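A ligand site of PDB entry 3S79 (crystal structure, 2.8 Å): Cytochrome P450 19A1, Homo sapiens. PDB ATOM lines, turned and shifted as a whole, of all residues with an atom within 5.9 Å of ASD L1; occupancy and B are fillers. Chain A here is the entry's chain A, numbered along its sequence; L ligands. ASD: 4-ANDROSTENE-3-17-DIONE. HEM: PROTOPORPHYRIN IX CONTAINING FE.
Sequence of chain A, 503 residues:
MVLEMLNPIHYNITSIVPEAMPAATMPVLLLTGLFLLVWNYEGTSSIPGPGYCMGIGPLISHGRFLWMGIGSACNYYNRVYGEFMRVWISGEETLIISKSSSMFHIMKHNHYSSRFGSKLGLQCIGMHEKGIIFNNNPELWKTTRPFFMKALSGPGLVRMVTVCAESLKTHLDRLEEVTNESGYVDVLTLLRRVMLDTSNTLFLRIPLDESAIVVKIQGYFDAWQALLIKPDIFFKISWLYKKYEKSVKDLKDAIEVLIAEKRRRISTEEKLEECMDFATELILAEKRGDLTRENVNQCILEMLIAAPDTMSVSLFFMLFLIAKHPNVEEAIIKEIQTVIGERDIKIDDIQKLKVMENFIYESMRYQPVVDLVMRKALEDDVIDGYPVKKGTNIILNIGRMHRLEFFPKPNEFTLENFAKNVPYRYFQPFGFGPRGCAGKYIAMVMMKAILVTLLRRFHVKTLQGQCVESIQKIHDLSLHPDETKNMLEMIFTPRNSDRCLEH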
ATOM      1  N   ARG A 115      12.326  15.763  20.559  1.00  0.00           N
ATOM      2  CA  ARG A 115      13.091  14.852  21.421  1.00  0.00           C
ATOM      3  C   ARG A 115      12.382  14.859  22.776  1.00  0.00           C
ATOM      4  O   ARG A 115      11.233  15.298  22.871  1.00  0.00           O
ATOM      5  CB  ARG A 115      14.548  15.297  21.571  1.00  0.00           C
ATOM      6  CG  ARG A 115      15.221  15.645  20.267  1.00  0.00           C
ATOM      7  CD  ARG A 115      16.731  15.521  20.348  1.00  0.00           C
ATOM      8  NE  ARG A 115      17.330  15.907  19.071  1.00  0.00           N
ATOM      9  CZ  ARG A 115      17.488  15.091  18.026  1.00  0.00           C
ATOM     10  NH1 ARG A 115      17.133  13.808  18.101  1.00  0.00           N
ATOM     11  NH2 ARG A 115      18.029  15.550  16.900  1.00  0.00           N
ATOM     12  N   ILE A 133      19.118  21.438  19.602  1.00  0.00           N
ATOM     13  CA  ILE A 133      19.410  20.029  19.873  1.00  0.00           C
ATOM     14  C   ILE A 133      18.305  19.379  20.699  1.00  0.00           C
ATOM     15  O   ILE A 133      17.709  18.397  20.270  1.00  0.00           O
ATOM     16  CB  ILE A 133      20.786  19.823  20.539  1.00  0.00           C
ATOM     17  CG1 ILE A 133      21.881  20.534  19.759  1.00  0.00           C
ATOM     18  CG2 ILE A 133      21.124  18.337  20.619  1.00  0.00           C
ATOM     19  CD1 ILE A 133      23.203  20.597  20.507  1.00  0.00           C
ATOM     20  N   PHE A 134      18.034  19.932  21.871  1.00  0.00           N
ATOM     21  CA  PHE A 134      16.982  19.398  22.726  1.00  0.00           C
ATOM     22  C   PHE A 134      15.843  20.405  22.944  1.00  0.00           C
ATOM     23  O   PHE A 134      15.146  20.369  23.962  1.00  0.00           O
ATOM     24  CB  PHE A 134      17.544  18.872  24.054  1.00  0.00           C
ATOM     25  CG  PHE A 134      17.996  17.439  23.986  1.00  0.00           C
ATOM     26  CD1 PHE A 134      19.267  17.111  23.544  1.00  0.00           C
ATOM     27  CD2 PHE A 134      17.130  16.410  24.344  1.00  0.00           C
ATOM     28  CE1 PHE A 134      19.681  15.781  23.457  1.00  0.00           C
ATOM     29  CE2 PHE A 134      17.536  15.075  24.261  1.00  0.00           C
ATOM     30  CZ  PHE A 134      18.811  14.761  23.818  1.00  0.00           C
ATOM     31  N   PHE A 221      29.108  19.139  28.755  1.00  0.00           N
ATOM     32  CA  PHE A 221      28.609  17.858  28.323  1.00  0.00           C
ATOM     33  C   PHE A 221      28.271  16.938  29.488  1.00  0.00           C
ATOM     34  O   PHE A 221      27.226  16.278  29.461  1.00  0.00           O
ATOM     35  CB  PHE A 221      29.557  17.156  27.349  1.00  0.00           C
ATOM     36  CG  PHE A 221      28.966  15.913  26.751  1.00  0.00           C
ATOM     37  CD1 PHE A 221      28.157  15.993  25.622  1.00  0.00           C
ATOM     38  CD2 PHE A 221      29.177  14.672  27.337  1.00  0.00           C
ATOM     39  CE1 PHE A 221      27.593  14.838  25.069  1.00  0.00           C
ATOM     40  CE2 PHE A 221      28.618  13.516  26.792  1.00  0.00           C
ATOM     41  CZ  PHE A 221      27.818  13.602  25.658  1.00  0.00           C
ATOM     42  N   TRP A 224      24.956  18.029  30.936  1.00  0.00           N
ATOM     43  CA  TRP A 224      23.942  17.626  29.966  1.00  0.00           C
ATOM     44  C   TRP A 224      23.651  16.135  30.098  1.00  0.00           C
ATOM     45  O   TRP A 224      22.509  15.735  30.328  1.00  0.00           O
ATOM     46  CB  TRP A 224      24.453  18.003  28.567  1.00  0.00           C
ATOM     47  CG  TRP A 224      23.605  17.624  27.399  1.00  0.00           C
ATOM     48  CD1 TRP A 224      22.343  17.098  27.404  1.00  0.00           C
ATOM     49  CD2 TRP A 224      23.957  17.779  26.016  1.00  0.00           C
ATOM     50  NE1 TRP A 224      21.898  16.899  26.115  1.00  0.00           N
ATOM     51  CE2 TRP A 224      22.872  17.312  25.249  1.00  0.00           C
ATOM     52  CE3 TRP A 224      25.095  18.274  25.356  1.00  0.00           C
ATOM     53  CZ2 TRP A 224      22.888  17.316  23.846  1.00  0.00           C
ATOM     54  CZ3 TRP A 224      25.117  18.278  23.962  1.00  0.00           C
ATOM     55  CH2 TRP A 224      24.008  17.791  23.223  1.00  0.00           C
ATOM     56  N   GLU A 302      25.409  26.124  21.359  1.00  0.00           N
ATOM     57  CA  GLU A 302      25.177  24.795  20.768  1.00  0.00           C
ATOM     58  C   GLU A 302      26.032  24.601  19.513  1.00  0.00           C
ATOM     59  O   GLU A 302      26.588  23.530  19.278  1.00  0.00           O
ATOM     60  CB  GLU A 302      23.687  24.575  20.479  1.00  0.00           C
ATOM     61  CG  GLU A 302      22.836  24.459  21.744  1.00  0.00           C
ATOM     62  CD  GLU A 302      21.434  23.893  21.516  1.00  0.00           C
ATOM     63  OE1 GLU A 302      21.067  23.573  20.350  1.00  0.00           O
ATOM     64  OE2 GLU A 302      20.672  23.768  22.513  1.00  0.00           O
ATOM     65  N   ILE A 305      29.779  23.811  20.577  1.00  0.00           N
ATOM     66  CA  ILE A 305      30.096  22.575  21.285  1.00  0.00           C
ATOM     67  C   ILE A 305      29.951  21.364  20.384  1.00  0.00           C
ATOM     68  O   ILE A 305      30.567  20.331  20.629  1.00  0.00           O
ATOM     69  CB  ILE A 305      29.230  22.405  22.558  1.00  0.00           C
ATOM     70  CG1 ILE A 305      27.745  22.242  22.208  1.00  0.00           C
ATOM     71  CG2 ILE A 305      29.469  23.570  23.515  1.00  0.00           C
ATOM     72  CD1 ILE A 305      26.870  21.738  23.341  1.00  0.00           C
ATOM     73  N   ALA A 306      29.137  21.503  19.345  1.00  0.00           N
ATOM     74  CA  ALA A 306      28.714  20.357  18.539  1.00  0.00           C
ATOM     75  C   ALA A 306      29.893  19.539  18.010  1.00  0.00           C
ATOM     76  O   ALA A 306      29.965  18.338  18.257  1.00  0.00           O
ATOM     77  CB  ALA A 306      27.788  20.793  17.418  1.00  0.00           C
ATOM     78  N   ALA A 307      30.811  20.195  17.300  1.00  0.00           N
ATOM     79  CA  ALA A 307      31.960  19.491  16.734  1.00  0.00           C
ATOM     80  C   ALA A 307      32.937  18.967  17.806  1.00  0.00           C
ATOM     81  O   ALA A 307      33.265  17.781  17.793  1.00  0.00           O
ATOM     82  CB  ALA A 307      32.662  20.356  15.695  1.00  0.00           C
ATOM     83  N   ASP A 309      32.221  18.027  20.740  1.00  0.00           N
ATOM     84  CA  ASP A 309      31.594  16.898  21.404  1.00  0.00           C
ATOM     85  C   ASP A 309      31.707  15.610  20.590  1.00  0.00           C
ATOM     86  O   ASP A 309      32.132  14.585  21.112  1.00  0.00           O
ATOM     87  CB  ASP A 309      30.120  17.185  21.703  1.00  0.00           C
ATOM     88  CG  ASP A 309      29.929  18.143  22.860  1.00  0.00           C
ATOM     89  OD1 ASP A 309      30.872  18.315  23.677  1.00  0.00           O
ATOM     90  OD2 ASP A 309      28.827  18.720  22.978  1.00  0.00           O
ATOM     91  N   THR A 310      31.356  15.684  19.320  1.00  0.00           N
ATOM     92  CA  THR A 310      31.152  14.487  18.508  1.00  0.00           C
ATOM     93  C   THR A 310      32.257  14.182  17.503  1.00  0.00           C
ATOM     94  O   THR A 310      32.658  13.033  17.369  1.00  0.00           O
ATOM     95  CB  THR A 310      29.812  14.539  17.764  1.00  0.00           C
ATOM     96  OG1 THR A 310      29.597  15.875  17.268  1.00  0.00           O
ATOM     97  CG2 THR A 310      28.683  14.184  18.700  1.00  0.00           C
ATOM     98  N   VAL A 370      27.554   8.430  18.329  1.00  0.00           N
ATOM     99  CA  VAL A 370      26.134   8.702  18.470  1.00  0.00           C
ATOM    100  C   VAL A 370      25.341   7.481  18.022  1.00  0.00           C
ATOM    101  O   VAL A 370      24.860   7.396  16.894  1.00  0.00           O
ATOM    102  CB  VAL A 370      25.724   9.959  17.681  1.00  0.00           C
ATOM    103  CG1 VAL A 370      24.332  10.394  18.088  1.00  0.00           C
ATOM    104  CG2 VAL A 370      26.716  11.089  17.906  1.00  0.00           C
ATOM    105  N   LEU A 372      22.587   6.340  19.480  1.00  0.00           N
ATOM    106  CA  LEU A 372      21.158   6.412  19.802  1.00  0.00           C
ATOM    107  C   LEU A 372      20.559   7.793  19.594  1.00  0.00           C
ATOM    108  O   LEU A 372      21.209   8.801  19.841  1.00  0.00           O
ATOM    109  CB  LEU A 372      20.885   5.894  21.215  1.00  0.00           C
ATOM    110  CG  LEU A 372      21.534   6.551  22.419  1.00  0.00           C
ATOM    111  CD1 LEU A 372      20.642   7.634  23.005  1.00  0.00           C
ATOM    112  CD2 LEU A 372      21.811   5.505  23.463  1.00  0.00           C
ATOM    113  N   VAL A 373      19.317   7.799  19.120  1.00  0.00           N
ATOM    114  CA  VAL A 373      18.596   9.043  18.821  1.00  0.00           C
ATOM    115  C   VAL A 373      17.322   9.108  19.641  1.00  0.00           C
ATOM    116  O   VAL A 373      16.534   8.153  19.672  1.00  0.00           O
ATOM    117  CB  VAL A 373      18.259   9.147  17.311  1.00  0.00           C
ATOM    118  CG1 VAL A 373      17.545  10.463  17.010  1.00  0.00           C
ATOM    119  CG2 VAL A 373      19.516   9.038  16.464  1.00  0.00           C
ATOM    120  N   MET A 374      17.129  10.230  20.334  1.00  0.00           N
ATOM    121  CA  MET A 374      15.941  10.421  21.161  1.00  0.00           C
ATOM    122  C   MET A 374      14.857  11.219  20.427  1.00  0.00           C
ATOM    123  O   MET A 374      15.132  12.295  19.880  1.00  0.00           O
ATOM    124  CB  MET A 374      16.308  11.087  22.484  1.00  0.00           C
ATOM    125  CG  MET A 374      17.129  10.193  23.406  1.00  0.00           C
ATOM    126  SD  MET A 374      17.886  11.043  24.822  1.00  0.00           S
ATOM    127  CE  MET A 374      16.450  11.425  25.813  1.00  0.00           C
ATOM    128  N   ARG A 375      13.643  10.669  20.398  1.00  0.00           N
ATOM    129  CA  ARG A 375      12.490  11.323  19.767  1.00  0.00           C
ATOM    130  C   ARG A 375      11.231  11.265  20.634  1.00  0.00           C
ATOM    131  O   ARG A 375      11.206  10.601  21.679  1.00  0.00           O
ATOM    132  CB  ARG A 375      12.205  10.714  18.378  1.00  0.00           C
ATOM    133  CG  ARG A 375      13.342  10.813  17.366  1.00  0.00           C
ATOM    134  CD  ARG A 375      13.731  12.246  17.056  1.00  0.00           C
ATOM    135  NE  ARG A 375      14.554  12.354  15.846  1.00  0.00           N
ATOM    136  CZ  ARG A 375      14.063  12.568  14.627  1.00  0.00           C
ATOM    137  NH1 ARG A 375      12.755  12.699  14.445  1.00  0.00           N
ATOM    138  NH2 ARG A 375      14.879  12.665  13.579  1.00  0.00           N
ATOM    139  N   LEU A 477      24.840   8.923  27.188  1.00  0.00           N
ATOM    140  CA  LEU A 477      24.233   9.805  26.206  1.00  0.00           C
ATOM    141  C   LEU A 477      24.861   9.551  24.837  1.00  0.00           C
ATOM    142  O   LEU A 477      24.180   9.511  23.823  1.00  0.00           O
ATOM    143  CB  LEU A 477      24.431  11.276  26.596  1.00  0.00           C
ATOM    144  CG  LEU A 477      23.379  12.341  26.237  1.00  0.00           C
ATOM    145  CD1 LEU A 477      24.057  13.591  25.688  1.00  0.00           C
ATOM    146  CD2 LEU A 477      22.314  11.856  25.275  1.00  0.00           C
ATOM    147  N   SER A 478      26.182   9.397  24.828  1.00  0.00           N
ATOM    148  CA  SER A 478      26.901   8.983  23.647  1.00  0.00           C
ATOM    149  C   SER A 478      27.845   7.858  24.052  1.00  0.00           C
ATOM    150  O   SER A 478      27.933   7.507  25.226  1.00  0.00           O
ATOM    151  CB  SER A 478      27.668  10.154  23.009  1.00  0.00           C
ATOM    152  OG  SER A 478      28.722  10.622  23.834  1.00  0.00           O
HETATM  153  C1  ASD L   1      24.415  17.050  19.252  1.00  0.00           C
HETATM  154  C10 ASD L   1      24.648  15.550  19.511  1.00  0.00           C
HETATM  155  C11 ASD L   1      22.148  15.135  19.213  1.00  0.00           C
HETATM  156  C12 ASD L   1      20.872  14.534  19.805  1.00  0.00           C
HETATM  157  C13 ASD L   1      21.132  13.069  20.096  1.00  0.00           C
HETATM  158  C14 ASD L   1      22.246  12.987  21.150  1.00  0.00           C
HETATM  159  C15 ASD L   1      22.151  11.572  21.720  1.00  0.00           C
HETATM  160  C16 ASD L   1      20.643  11.360  21.868  1.00  0.00           C
HETATM  161  C17 ASD L   1      20.059  12.303  20.835  1.00  0.00           C
HETATM  162  C18 ASD L   1      21.433  12.292  18.811  1.00  0.00           C
HETATM  163  C19 ASD L   1      24.987  14.847  18.190  1.00  0.00           C
HETATM  164  C2  ASD L   1      25.710  17.854  19.138  1.00  0.00           C
HETATM  165  C3  ASD L   1      26.510  17.593  20.387  1.00  0.00           C
HETATM  166  C4  ASD L   1      26.612  16.332  20.889  1.00  0.00           C
HETATM  167  C5  ASD L   1      25.790  15.336  20.517  1.00  0.00           C
HETATM  168  C6  ASD L   1      25.992  13.968  21.129  1.00  0.00           C
HETATM  169  C7  ASD L   1      24.661  13.475  21.703  1.00  0.00           C
HETATM  170  C8  ASD L   1      23.575  13.527  20.640  1.00  0.00           C
HETATM  171  C9  ASD L   1      23.369  14.961  20.131  1.00  0.00           C
HETATM  172  O1  ASD L   1      27.070  18.543  20.936  1.00  0.00           O
HETATM  173  O2  ASD L   1      18.864  12.428  20.612  1.00  0.00           O
HETATM  174  CHA HEM L   2      21.771  15.984  15.603  1.00  0.00           C
HETATM  175  CHB HEM L   2      25.093  12.655  14.457  1.00  0.00           C
HETATM  176  CHC HEM L   2      28.274  16.201  13.691  1.00  0.00           C
HETATM  177  CHD HEM L   2      24.963  19.551  14.686  1.00  0.00           C
HETATM  178  C1A HEM L   2      22.371  14.777  15.321  1.00  0.00           C
HETATM  179  C2A HEM L   2      21.719  13.489  15.331  1.00  0.00           C
HETATM  180  C3A HEM L   2      22.632  12.570  15.003  1.00  0.00           C
HETATM  181  C4A HEM L   2      23.899  13.248  14.783  1.00  0.00           C
HETATM  182  CMA HEM L   2      22.405  11.041  14.884  1.00  0.00           C
HETATM  183  CAA HEM L   2      20.217  13.229  15.629  1.00  0.00           C
HETATM  184  CBA HEM L   2      19.448  13.416  14.333  1.00  0.00           C
HETATM  185  CGA HEM L   2      18.042  12.872  14.411  1.00  0.00           C
HETATM  186  O1A HEM L   2      17.328  13.100  15.437  1.00  0.00           O
HETATM  187  O2A HEM L   2      17.599  12.207  13.430  1.00  0.00           O
HETATM  188  C1B HEM L   2      26.276  13.314  14.257  1.00  0.00           C
HETATM  189  C2B HEM L   2      27.597  12.731  14.135  1.00  0.00           C
HETATM  190  C3B HEM L   2      28.467  13.727  13.917  1.00  0.00           C
HETATM  191  C4B HEM L   2      27.715  14.954  13.905  1.00  0.00           C
HETATM  192  CMB HEM L   2      27.924  11.227  14.221  1.00  0.00           C
HETATM  193  CAB HEM L   2      30.005  13.674  13.717  1.00  0.00           C
HETATM  194  CBB HEM L   2      30.616  12.602  13.213  1.00  0.00           C
HETATM  195  C1C HEM L   2      27.653  17.404  13.854  1.00  0.00           C
HETATM  196  C2C HEM L   2      28.260  18.697  13.633  1.00  0.00           C
HETATM  197  C3C HEM L   2      27.342  19.640  13.917  1.00  0.00           C
HETATM  198  C4C HEM L   2      26.132  18.950  14.316  1.00  0.00           C
HETATM  199  CMC HEM L   2      29.719  18.914  13.168  1.00  0.00           C
HETATM  200  CAC HEM L   2      27.487  21.177  13.837  1.00  0.00           C
HETATM  201  CBC HEM L   2      28.636  21.809  14.118  1.00  0.00           C
HETATM  202  C1D HEM L   2      23.810  18.919  15.084  1.00  0.00           C
HETATM  203  C2D HEM L   2      22.629  19.586  15.585  1.00  0.00           C
HETATM  204  C3D HEM L   2      21.625  18.473  15.877  1.00  0.00           C
HETATM  205  C4D HEM L   2      22.307  17.248  15.514  1.00  0.00           C
HETATM  206  CMD HEM L   2      22.447  21.106  15.776  1.00  0.00           C
HETATM  207  CAD HEM L   2      20.183  18.660  16.418  1.00  0.00           C
HETATM  208  CBD HEM L   2      19.262  18.707  15.207  1.00  0.00           C
HETATM  209  CGD HEM L   2      17.816  18.973  15.571  1.00  0.00           C
HETATM  210  O1D HEM L   2      17.130  19.719  14.831  1.00  0.00           O
HETATM  211  O2D HEM L   2      17.338  18.425  16.603  1.00  0.00           O
HETATM  212  NA  HEM L   2      23.692  14.603  14.960  1.00  0.00           N
HETATM  213  NB  HEM L   2      26.384  14.673  14.111  1.00  0.00           N
HETATM  214  NC  HEM L   2      26.345  17.586  14.242  1.00  0.00           N
HETATM  215  ND  HEM L   2      23.591  17.548  15.051  1.00  0.00           N
HETATM  216 FE   HEM L   2      25.010  16.088  14.540  1.00  0.00          FE
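NH1 of Arg 115 is in hydrogen-bond range of O2 of ASD L1, at 3.3 Å. The backbone NH of Met 374 sits at hydrogen-bond distance from an oxygen (O2) of ASD L1 (2.8 Å). An oxygen (O1) of ASD L1 sits close to the side-chain carboxylate (OD2) of Asp 309 (2.7 Å). An oxygen (O2A) of HEM L2 is in salt-bridge range of the guanidinium group (NH2) of Arg 375 (2.8 Å). O1A of HEM L2 lies within salt-bridge range of NH1 of Arg 115, 2.8 Å away.
Ile 133 touches ASD L1. CZ of Phe 134 touches O2 of ASD L1 (3.97 Å). CZ3 of Trp 224 touches O1 of ASD L1, at 3.6 Å. Ile 305 touches ASD L1. CA of Ala 306 touches O1 of ASD L1 (3.4 Å). Thr 310 touches ASD L1 (CG2 to C5, 3.6 Å). CG1 of Val 370 touches C18 of ASD L1, at 3.5 Å. Leu 372 touches ASD L1. C of Val 373 touches O2 of ASD L1 (3.8 Å). Leu 477 touches ASD L1. Hydrophobic or aromatic side chains within 4 Å of ASD L1: Ile 133, Phe 134, Trp 224, Ile 305, Ala 306, Val 370, Leu 372, Met 374 and Leu 477. Of the 18 residues printed, 13 come within 4 Å of ASD L1. Along chain A the residues within 4 Å of ASD L1 span positions 115 to 477. The nearest printed residue that does not touch ASD L1 is Phe 221 (4.3 Å).
The guanidinium group of Arg 115 is in hydrogen-bond range of the backbone carbonyl oxygen of Met 374 (3.1 Å). The guanidinium group (NE) of Arg 115 is in hydrogen-bond range of the backbone carbonyl oxygen (O) of Ile 133 (2.8 Å). OG1 of Thr 310 is in hydrogen-bond range of O of Ala 306, 2.7 Å away. The backbone NH (N) of Ile 133 is in hydrogen-bond range of the side-chain carboxylate (OE1) of Glu 302, at 3.0 Å.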
